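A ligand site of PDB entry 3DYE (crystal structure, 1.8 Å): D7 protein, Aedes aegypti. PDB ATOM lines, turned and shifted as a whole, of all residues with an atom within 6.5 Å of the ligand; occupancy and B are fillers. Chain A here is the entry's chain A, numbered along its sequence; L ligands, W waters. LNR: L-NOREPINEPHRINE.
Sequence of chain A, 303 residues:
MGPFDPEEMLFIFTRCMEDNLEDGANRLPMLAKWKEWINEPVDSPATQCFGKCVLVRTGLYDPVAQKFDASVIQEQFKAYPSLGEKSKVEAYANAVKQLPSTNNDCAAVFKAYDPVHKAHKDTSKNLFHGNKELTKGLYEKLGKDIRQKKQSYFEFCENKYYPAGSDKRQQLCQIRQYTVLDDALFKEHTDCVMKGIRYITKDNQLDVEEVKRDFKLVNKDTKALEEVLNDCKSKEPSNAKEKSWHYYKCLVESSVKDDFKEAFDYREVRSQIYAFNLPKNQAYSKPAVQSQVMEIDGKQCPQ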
ATOM      1  N   PHE A 154      32.510  22.503  -3.638  1.00  0.00           N
ATOM      2  CA  PHE A 154      31.903  23.831  -3.683  1.00  0.00           C
ATOM      3  C   PHE A 154      32.805  24.784  -4.455  1.00  0.00           C
ATOM      4  O   PHE A 154      32.327  25.528  -5.320  1.00  0.00           O
ATOM      5  CB  PHE A 154      31.668  24.379  -2.279  1.00  0.00           C
ATOM      6  CG  PHE A 154      30.490  23.758  -1.574  1.00  0.00           C
ATOM      7  CD1 PHE A 154      29.461  24.556  -1.099  1.00  0.00           C
ATOM      8  CD2 PHE A 154      30.417  22.379  -1.361  1.00  0.00           C
ATOM      9  CE1 PHE A 154      28.372  24.000  -0.430  1.00  0.00           C
ATOM     10  CE2 PHE A 154      29.329  21.815  -0.697  1.00  0.00           C
ATOM     11  CZ  PHE A 154      28.306  22.634  -0.235  1.00  0.00           C
ATOM     12  N   GLU A 155      34.100  24.743  -4.150  1.00  0.00           N
ATOM     13  CA  GLU A 155      35.094  25.566  -4.856  1.00  0.00           C
ATOM     14  C   GLU A 155      35.103  25.262  -6.351  1.00  0.00           C
ATOM     15  O   GLU A 155      35.172  26.185  -7.173  1.00  0.00           O
ATOM     16  CB  GLU A 155      36.502  25.344  -4.292  1.00  0.00           C
ATOM     17  CG  GLU A 155      37.565  26.196  -4.981  1.00  0.00           C
ATOM     18  CD  GLU A 155      38.972  25.720  -4.689  1.00  0.00           C
ATOM     19  OE1 GLU A 155      39.355  25.731  -3.491  1.00  0.00           O
ATOM     20  OE2 GLU A 155      39.685  25.346  -5.640  1.00  0.00           O
ATOM     21  N   CYS A 157      32.646  24.171  -8.256  1.00  0.00           N
ATOM     22  CA  CYS A 157      31.478  24.768  -8.914  1.00  0.00           C
ATOM     23  C   CYS A 157      31.574  26.299  -8.954  1.00  0.00           C
ATOM     24  O   CYS A 157      31.291  26.908  -9.977  1.00  0.00           O
ATOM     25  CB  CYS A 157      30.197  24.340  -8.226  1.00  0.00           C
ATOM     26  SG  CYS A 157      29.893  22.559  -8.340  1.00  0.00           S
ATOM     27  N   GLU A 158      31.972  26.885  -7.835  1.00  0.00           N
ATOM     28  CA  GLU A 158      32.120  28.341  -7.714  1.00  0.00           C
ATOM     29  C   GLU A 158      33.080  28.899  -8.773  1.00  0.00           C
ATOM     30  O   GLU A 158      32.793  29.920  -9.399  1.00  0.00           O
ATOM     31  CB  GLU A 158      32.611  28.724  -6.324  1.00  0.00           C
ATOM     32  CG  GLU A 158      31.551  28.596  -5.223  1.00  0.00           C
ATOM     33  CD  GLU A 158      32.119  28.784  -3.833  1.00  0.00           C
ATOM     34  OE1 GLU A 158      33.347  28.928  -3.694  1.00  0.00           O
ATOM     35  OE2 GLU A 158      31.322  28.804  -2.878  1.00  0.00           O
ATOM     36  N   LEU A 172      29.813  35.717  -5.119  1.00  0.00           N
ATOM     37  CA  LEU A 172      30.110  34.673  -4.123  1.00  0.00           C
ATOM     38  C   LEU A 172      29.970  35.159  -2.685  1.00  0.00           C
ATOM     39  O   LEU A 172      29.714  34.363  -1.786  1.00  0.00           O
ATOM     40  CB  LEU A 172      31.484  34.059  -4.362  1.00  0.00           C
ATOM     41  CG  LEU A 172      31.706  33.246  -5.649  1.00  0.00           C
ATOM     42  CD1 LEU A 172      33.117  32.684  -5.688  1.00  0.00           C
ATOM     43  CD2 LEU A 172      30.688  32.126  -5.820  1.00  0.00           C
ATOM     44  N   GLN A 174      27.539  36.977  -1.419  1.00  0.00           N
ATOM     45  CA  GLN A 174      26.155  36.683  -1.045  1.00  0.00           C
ATOM     46  C   GLN A 174      25.860  35.192  -1.109  1.00  0.00           C
ATOM     47  O   GLN A 174      25.234  34.644  -0.194  1.00  0.00           O
ATOM     48  CB  GLN A 174      25.188  37.423  -1.960  1.00  0.00           C
ATOM     49  CG  GLN A 174      24.964  38.868  -1.603  1.00  0.00           C
ATOM     50  CD  GLN A 174      23.770  39.460  -2.331  1.00  0.00           C
ATOM     51  OE1 GLN A 174      23.237  38.741  -3.314  1.00  0.00           O
ATOM     52  NE2 GLN A 174      23.313  40.561  -2.004  1.00  0.00           N
ATOM     53  N   ILE A 175      26.287  34.545  -2.186  1.00  0.00           N
ATOM     54  CA  ILE A 175      26.019  33.121  -2.409  1.00  0.00           C
ATOM     55  C   ILE A 175      26.483  32.294  -1.211  1.00  0.00           C
ATOM     56  O   ILE A 175      25.733  31.461  -0.701  1.00  0.00           O
ATOM     57  CB  ILE A 175      26.633  32.617  -3.743  1.00  0.00           C
ATOM     58  CG1 ILE A 175      25.817  33.177  -4.918  1.00  0.00           C
ATOM     59  CG2 ILE A 175      26.659  31.084  -3.799  1.00  0.00           C
ATOM     60  CD1 ILE A 175      26.483  33.073  -6.259  1.00  0.00           C
ATOM     61  N   ARG A 176      27.706  32.555  -0.754  1.00  0.00           N
ATOM     62  CA  ARG A 176      28.274  31.791   0.357  1.00  0.00           C
ATOM     63  C   ARG A 176      27.589  32.071   1.700  1.00  0.00           C
ATOM     64  O   ARG A 176      27.809  31.341   2.681  1.00  0.00           O
ATOM     65  CB  ARG A 176      29.790  31.996   0.435  1.00  0.00           C
ATOM     66  CG  ARG A 176      30.538  31.351  -0.740  1.00  0.00           C
ATOM     67  CD  ARG A 176      32.042  31.251  -0.503  1.00  0.00           C
ATOM     68  NE  ARG A 176      32.338  30.508   0.710  1.00  0.00           N
ATOM     69  CZ  ARG A 176      32.377  29.181   0.819  1.00  0.00           C
ATOM     70  NH1 ARG A 176      32.138  28.415  -0.243  1.00  0.00           N
ATOM     71  NH2 ARG A 176      32.662  28.623   1.983  1.00  0.00           N
ATOM     72  N   GLN A 177      26.764  33.115   1.740  1.00  0.00           N
ATOM     73  CA  GLN A 177      25.953  33.412   2.930  1.00  0.00           C
ATOM     74  C   GLN A 177      24.504  32.957   2.749  1.00  0.00           C
ATOM     75  O   GLN A 177      23.580  33.511   3.358  1.00  0.00           O
ATOM     76  CB  GLN A 177      26.046  34.896   3.279  1.00  0.00           C
ATOM     77  CG  GLN A 177      27.449  35.357   3.649  1.00  0.00           C
ATOM     78  CD  GLN A 177      28.134  34.444   4.653  1.00  0.00           C
ATOM     79  OE1 GLN A 177      27.583  34.141   5.714  1.00  0.00           O
ATOM     80  NE2 GLN A 177      29.344  34.004   4.328  1.00  0.00           N
ATOM     81  N   TYR A 178      24.328  31.925   1.926  1.00  0.00           N
ATOM     82  CA  TYR A 178      23.026  31.283   1.664  1.00  0.00           C
ATOM     83  C   TYR A 178      21.943  32.204   1.086  1.00  0.00           C
ATOM     84  O   TYR A 178      20.750  31.975   1.287  1.00  0.00           O
ATOM     85  CB  TYR A 178      22.521  30.528   2.897  1.00  0.00           C
ATOM     86  CG  TYR A 178      23.384  29.336   3.224  1.00  0.00           C
ATOM     87  CD1 TYR A 178      23.160  28.098   2.624  1.00  0.00           C
ATOM     88  CD2 TYR A 178      24.446  29.448   4.119  1.00  0.00           C
ATOM     89  CE1 TYR A 178      23.954  27.001   2.904  1.00  0.00           C
ATOM     90  CE2 TYR A 178      25.254  28.354   4.417  1.00  0.00           C
ATOM     91  CZ  TYR A 178      25.001  27.130   3.809  1.00  0.00           C
ATOM     92  OH  TYR A 178      25.801  26.055   4.095  1.00  0.00           O
ATOM     93  N   PHE A 186      22.902  31.036 -11.519  1.00  0.00           N
ATOM     94  CA  PHE A 186      22.828  30.490 -10.171  1.00  0.00           C
ATOM     95  C   PHE A 186      22.155  29.128 -10.127  1.00  0.00           C
ATOM     96  O   PHE A 186      22.573  28.252  -9.361  1.00  0.00           O
ATOM     97  CB  PHE A 186      22.129  31.435  -9.200  1.00  0.00           C
ATOM     98  CG  PHE A 186      22.143  30.951  -7.772  1.00  0.00           C
ATOM     99  CD1 PHE A 186      23.321  30.944  -7.049  1.00  0.00           C
ATOM    100  CD2 PHE A 186      20.970  30.498  -7.161  1.00  0.00           C
ATOM    101  CE1 PHE A 186      23.349  30.488  -5.721  1.00  0.00           C
ATOM    102  CE2 PHE A 186      20.976  30.053  -5.852  1.00  0.00           C
ATOM    103  CZ  PHE A 186      22.169  30.039  -5.116  1.00  0.00           C
ATOM    104  N   HIS A 189      24.764  26.705 -11.264  1.00  0.00           N
ATOM    105  CA  HIS A 189      25.734  26.545 -10.197  1.00  0.00           C
ATOM    106  C   HIS A 189      25.178  25.621  -9.095  1.00  0.00           C
ATOM    107  O   HIS A 189      25.865  24.711  -8.635  1.00  0.00           O
ATOM    108  CB  HIS A 189      26.113  27.903  -9.616  1.00  0.00           C
ATOM    109  CG  HIS A 189      26.855  27.818  -8.320  1.00  0.00           C
ATOM    110  ND1 HIS A 189      28.182  27.429  -8.247  1.00  0.00           N
ATOM    111  CD2 HIS A 189      26.457  28.055  -7.044  1.00  0.00           C
ATOM    112  CE1 HIS A 189      28.564  27.435  -6.985  1.00  0.00           C
ATOM    113  NE2 HIS A 189      27.544  27.804  -6.231  1.00  0.00           N
ATOM    114  N   THR A 190      23.938  25.858  -8.697  1.00  0.00           N
ATOM    115  CA  THR A 190      23.317  25.076  -7.638  1.00  0.00           C
ATOM    116  C   THR A 190      23.125  23.622  -8.083  1.00  0.00           C
ATOM    117  O   THR A 190      23.262  22.698  -7.275  1.00  0.00           O
ATOM    118  CB  THR A 190      22.006  25.746  -7.163  1.00  0.00           C
ATOM    119  OG1 THR A 190      22.319  27.055  -6.663  1.00  0.00           O
ATOM    120  CG2 THR A 190      21.371  24.941  -6.052  1.00  0.00           C
ATOM    121  N   VAL A 193      26.513  22.009  -7.572  1.00  0.00           N
ATOM    122  CA  VAL A 193      26.791  21.709  -6.159  1.00  0.00           C
ATOM    123  C   VAL A 193      25.935  20.540  -5.677  1.00  0.00           C
ATOM    124  O   VAL A 193      26.454  19.576  -5.113  1.00  0.00           O
ATOM    125  CB  VAL A 193      26.620  22.950  -5.237  1.00  0.00           C
ATOM    126  CG1 VAL A 193      26.825  22.570  -3.765  1.00  0.00           C
ATOM    127  CG2 VAL A 193      27.614  24.046  -5.627  1.00  0.00           C
ATOM    128  N   TYR A 248      17.356  23.215  -3.091  1.00  0.00           N
ATOM    129  CA  TYR A 248      18.251  24.101  -2.346  1.00  0.00           C
ATOM    130  C   TYR A 248      17.472  25.284  -1.757  1.00  0.00           C
ATOM    131  O   TYR A 248      17.549  25.551  -0.548  1.00  0.00           O
ATOM    132  CB  TYR A 248      19.376  24.598  -3.254  1.00  0.00           C
ATOM    133  CG  TYR A 248      20.309  25.581  -2.565  1.00  0.00           C
ATOM    134  CD1 TYR A 248      21.286  25.135  -1.681  1.00  0.00           C
ATOM    135  CD2 TYR A 248      20.198  26.956  -2.792  1.00  0.00           C
ATOM    136  CE1 TYR A 248      22.140  26.029  -1.046  1.00  0.00           C
ATOM    137  CE2 TYR A 248      21.037  27.865  -2.165  1.00  0.00           C
ATOM    138  CZ  TYR A 248      22.009  27.389  -1.291  1.00  0.00           C
ATOM    139  OH  TYR A 248      22.835  28.289  -0.669  1.00  0.00           O
ATOM    140  N   LYS A 261      22.036  24.531   6.935  1.00  0.00           N
ATOM    141  CA  LYS A 261      23.267  25.295   6.756  1.00  0.00           C
ATOM    142  C   LYS A 261      24.428  24.650   7.526  1.00  0.00           C
ATOM    143  O   LYS A 261      25.559  24.599   7.030  1.00  0.00           O
ATOM    144  CB  LYS A 261      23.069  26.752   7.170  1.00  0.00           C
ATOM    145  CG  LYS A 261      22.129  27.525   6.226  1.00  0.00           C
ATOM    146  CD  LYS A 261      21.786  28.902   6.768  1.00  0.00           C
ATOM    147  CE  LYS A 261      20.652  29.556   5.987  1.00  0.00           C
ATOM    148  NZ  LYS A 261      20.500  30.982   6.380  1.00  0.00           N
ATOM    149  N   PHE A 264      25.352  21.401   5.591  1.00  0.00           N
ATOM    150  CA  PHE A 264      25.898  21.753   4.267  1.00  0.00           C
ATOM    151  C   PHE A 264      27.328  22.287   4.432  1.00  0.00           C
ATOM    152  O   PHE A 264      28.221  21.933   3.657  1.00  0.00           O
ATOM    153  CB  PHE A 264      24.991  22.821   3.627  1.00  0.00           C
ATOM    154  CG  PHE A 264      24.905  22.784   2.113  1.00  0.00           C
ATOM    155  CD1 PHE A 264      24.450  21.643   1.446  1.00  0.00           C
ATOM    156  CD2 PHE A 264      25.208  23.919   1.378  1.00  0.00           C
ATOM    157  CE1 PHE A 264      24.339  21.632   0.057  1.00  0.00           C
ATOM    158  CE2 PHE A 264      25.082  23.922  -0.018  1.00  0.00           C
ATOM    159  CZ  PHE A 264      24.656  22.767  -0.678  1.00  0.00           C
ATOM    160  N   ASP A 265      27.535  23.123   5.456  1.00  0.00           N
ATOM    161  CA  ASP A 265      28.879  23.627   5.788  1.00  0.00           C
ATOM    162  C   ASP A 265      29.866  22.500   6.103  1.00  0.00           C
ATOM    163  O   ASP A 265      31.000  22.510   5.622  1.00  0.00           O
ATOM    164  CB  ASP A 265      28.833  24.611   6.979  1.00  0.00           C
ATOM    165  CG  ASP A 265      28.306  25.997   6.592  1.00  0.00           C
ATOM    166  OD1 ASP A 265      28.089  26.274   5.390  1.00  0.00           O
ATOM    167  OD2 ASP A 265      28.112  26.815   7.521  1.00  0.00           O
ATOM    168  N   GLU A 268      30.703  20.639   2.916  1.00  0.00           N
ATOM    169  CA  GLU A 268      31.716  21.395   2.167  1.00  0.00           C
ATOM    170  C   GLU A 268      33.134  21.046   2.616  1.00  0.00           C
ATOM    171  O   GLU A 268      34.002  20.757   1.791  1.00  0.00           O
ATOM    172  CB  GLU A 268      31.485  22.897   2.284  1.00  0.00           C
ATOM    173  CG  GLU A 268      32.377  23.723   1.355  1.00  0.00           C
ATOM    174  CD  GLU A 268      32.301  25.216   1.579  1.00  0.00           C
ATOM    175  OE1 GLU A 268      31.486  25.675   2.403  1.00  0.00           O
ATOM    176  OE2 GLU A 268      33.067  25.957   0.918  1.00  0.00           O
ATOM    177  N   VAL A 293      35.095  27.231   7.414  1.00  0.00           N
ATOM    178  CA  VAL A 293      34.172  27.757   6.412  1.00  0.00           C
ATOM    179  C   VAL A 293      34.270  29.277   6.297  1.00  0.00           C
ATOM    180  O   VAL A 293      34.205  29.822   5.196  1.00  0.00           O
ATOM    181  CB  VAL A 293      32.710  27.277   6.677  1.00  0.00           C
ATOM    182  CG1 VAL A 293      31.717  27.983   5.758  1.00  0.00           C
ATOM    183  CG2 VAL A 293      32.609  25.772   6.491  1.00  0.00           C
ATOM    184  N   ASP A 297      35.215  31.543   3.124  1.00  0.00           N
ATOM    185  CA  ASP A 297      34.444  32.745   2.810  1.00  0.00           C
ATOM    186  C   ASP A 297      35.353  33.924   2.467  1.00  0.00           C
ATOM    187  O   ASP A 297      35.142  34.617   1.471  1.00  0.00           O
ATOM    188  CB  ASP A 297      33.528  33.141   3.982  1.00  0.00           C
ATOM    189  CG  ASP A 297      32.388  32.152   4.208  1.00  0.00           C
ATOM    190  OD1 ASP A 297      32.235  31.196   3.416  1.00  0.00           O
ATOM    191  OD2 ASP A 297      31.637  32.349   5.190  1.00  0.00           O
HETATM  192  OAC LNR L   1      28.550  28.007  -3.642  1.00  0.00           O
HETATM  193  CAJ LNR L   1      27.695  27.806  -2.609  1.00  0.00           C
HETATM  194  CAG LNR L   1      28.131  27.851  -1.290  1.00  0.00           C
HETATM  195  CAI LNR L   1      26.354  27.556  -2.838  1.00  0.00           C
HETATM  196  OAB LNR L   1      25.840  27.505  -4.100  1.00  0.00           O
HETATM  197  CAE LNR L   1      25.512  27.359  -1.752  1.00  0.00           C
HETATM  198  CAF LNR L   1      25.964  27.400  -0.537  1.00  0.00           C
HETATM  199  CAK LNR L   1      27.206  27.629  -0.269  1.00  0.00           C
HETATM  200  CAL LNR L   1      27.599  27.644   1.166  1.00  0.00           C
HETATM  201  OAD LNR L   1      27.131  28.862   1.736  1.00  0.00           O
HETATM  202  CAH LNR L   1      29.113  27.522   1.363  1.00  0.00           C
HETATM  203  NAA LNR L   1      29.390  27.150   2.739  1.00  0.00           N
HETATM  204  O   HOH W   1      29.706  29.747   3.717  1.00  0.00           O
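NAA of the ligand is in salt-bridge range of OE1 of Glu 268.
OAD of the ligand lies within hydrogen-bond range of O of Arg 176.
NE2 of His 189 lies within hydrogen-bond range of OAB of the ligand.
OE2 of Glu 158 sits at hydrogen-bond distance from OAC of the ligand (3.0 Å).
OD1 of Asp 265 is in salt-bridge range of NAA of the ligand.
Water W1 lies within hydrogen-bond range of O of Arg 176, NAA of the ligand and OD1 of Asp 297.
CD1 of Phe 154 touches CAG of the ligand, at 3.6 Å.
CG2 of Ile 175 touches OAC of the ligand, 3.6 Å away.
Tyr 178 touches the ligand (CE2 to OAD, 3.3 Å).
Tyr 248 touches the ligand (OH to CAE, 3.0 Å).
Phe 264 touches the ligand (CE2 to CAF, 3.6 Å).
CG1 of Val 293 touches NAA of the ligand (3.9 Å).
The nearest printed residue that does not touch the ligand is Val 193 (4.2 Å).
The side-chain carboxylate of Glu 268 is in salt-bridge range of the guanidinium group of Arg 176, 2.9 Å away.
NH1 of Arg 176 lies within salt-bridge range of OE2 of Glu 158.
NE of Arg 176 is in salt-bridge range of OD1 of Asp 297 (2.8 Å).
The side-chain hydroxyl (OH) of Tyr 178 lies within hydrogen-bond range of the side-chain carboxylate (OD1) of Asp 265 (2.6 Å).
The side-chain hydroxyl (OH) of Tyr 178 sits at hydrogen-bond distance from the backbone carbonyl oxygen (O) of Lys 261 (3.3 Å).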
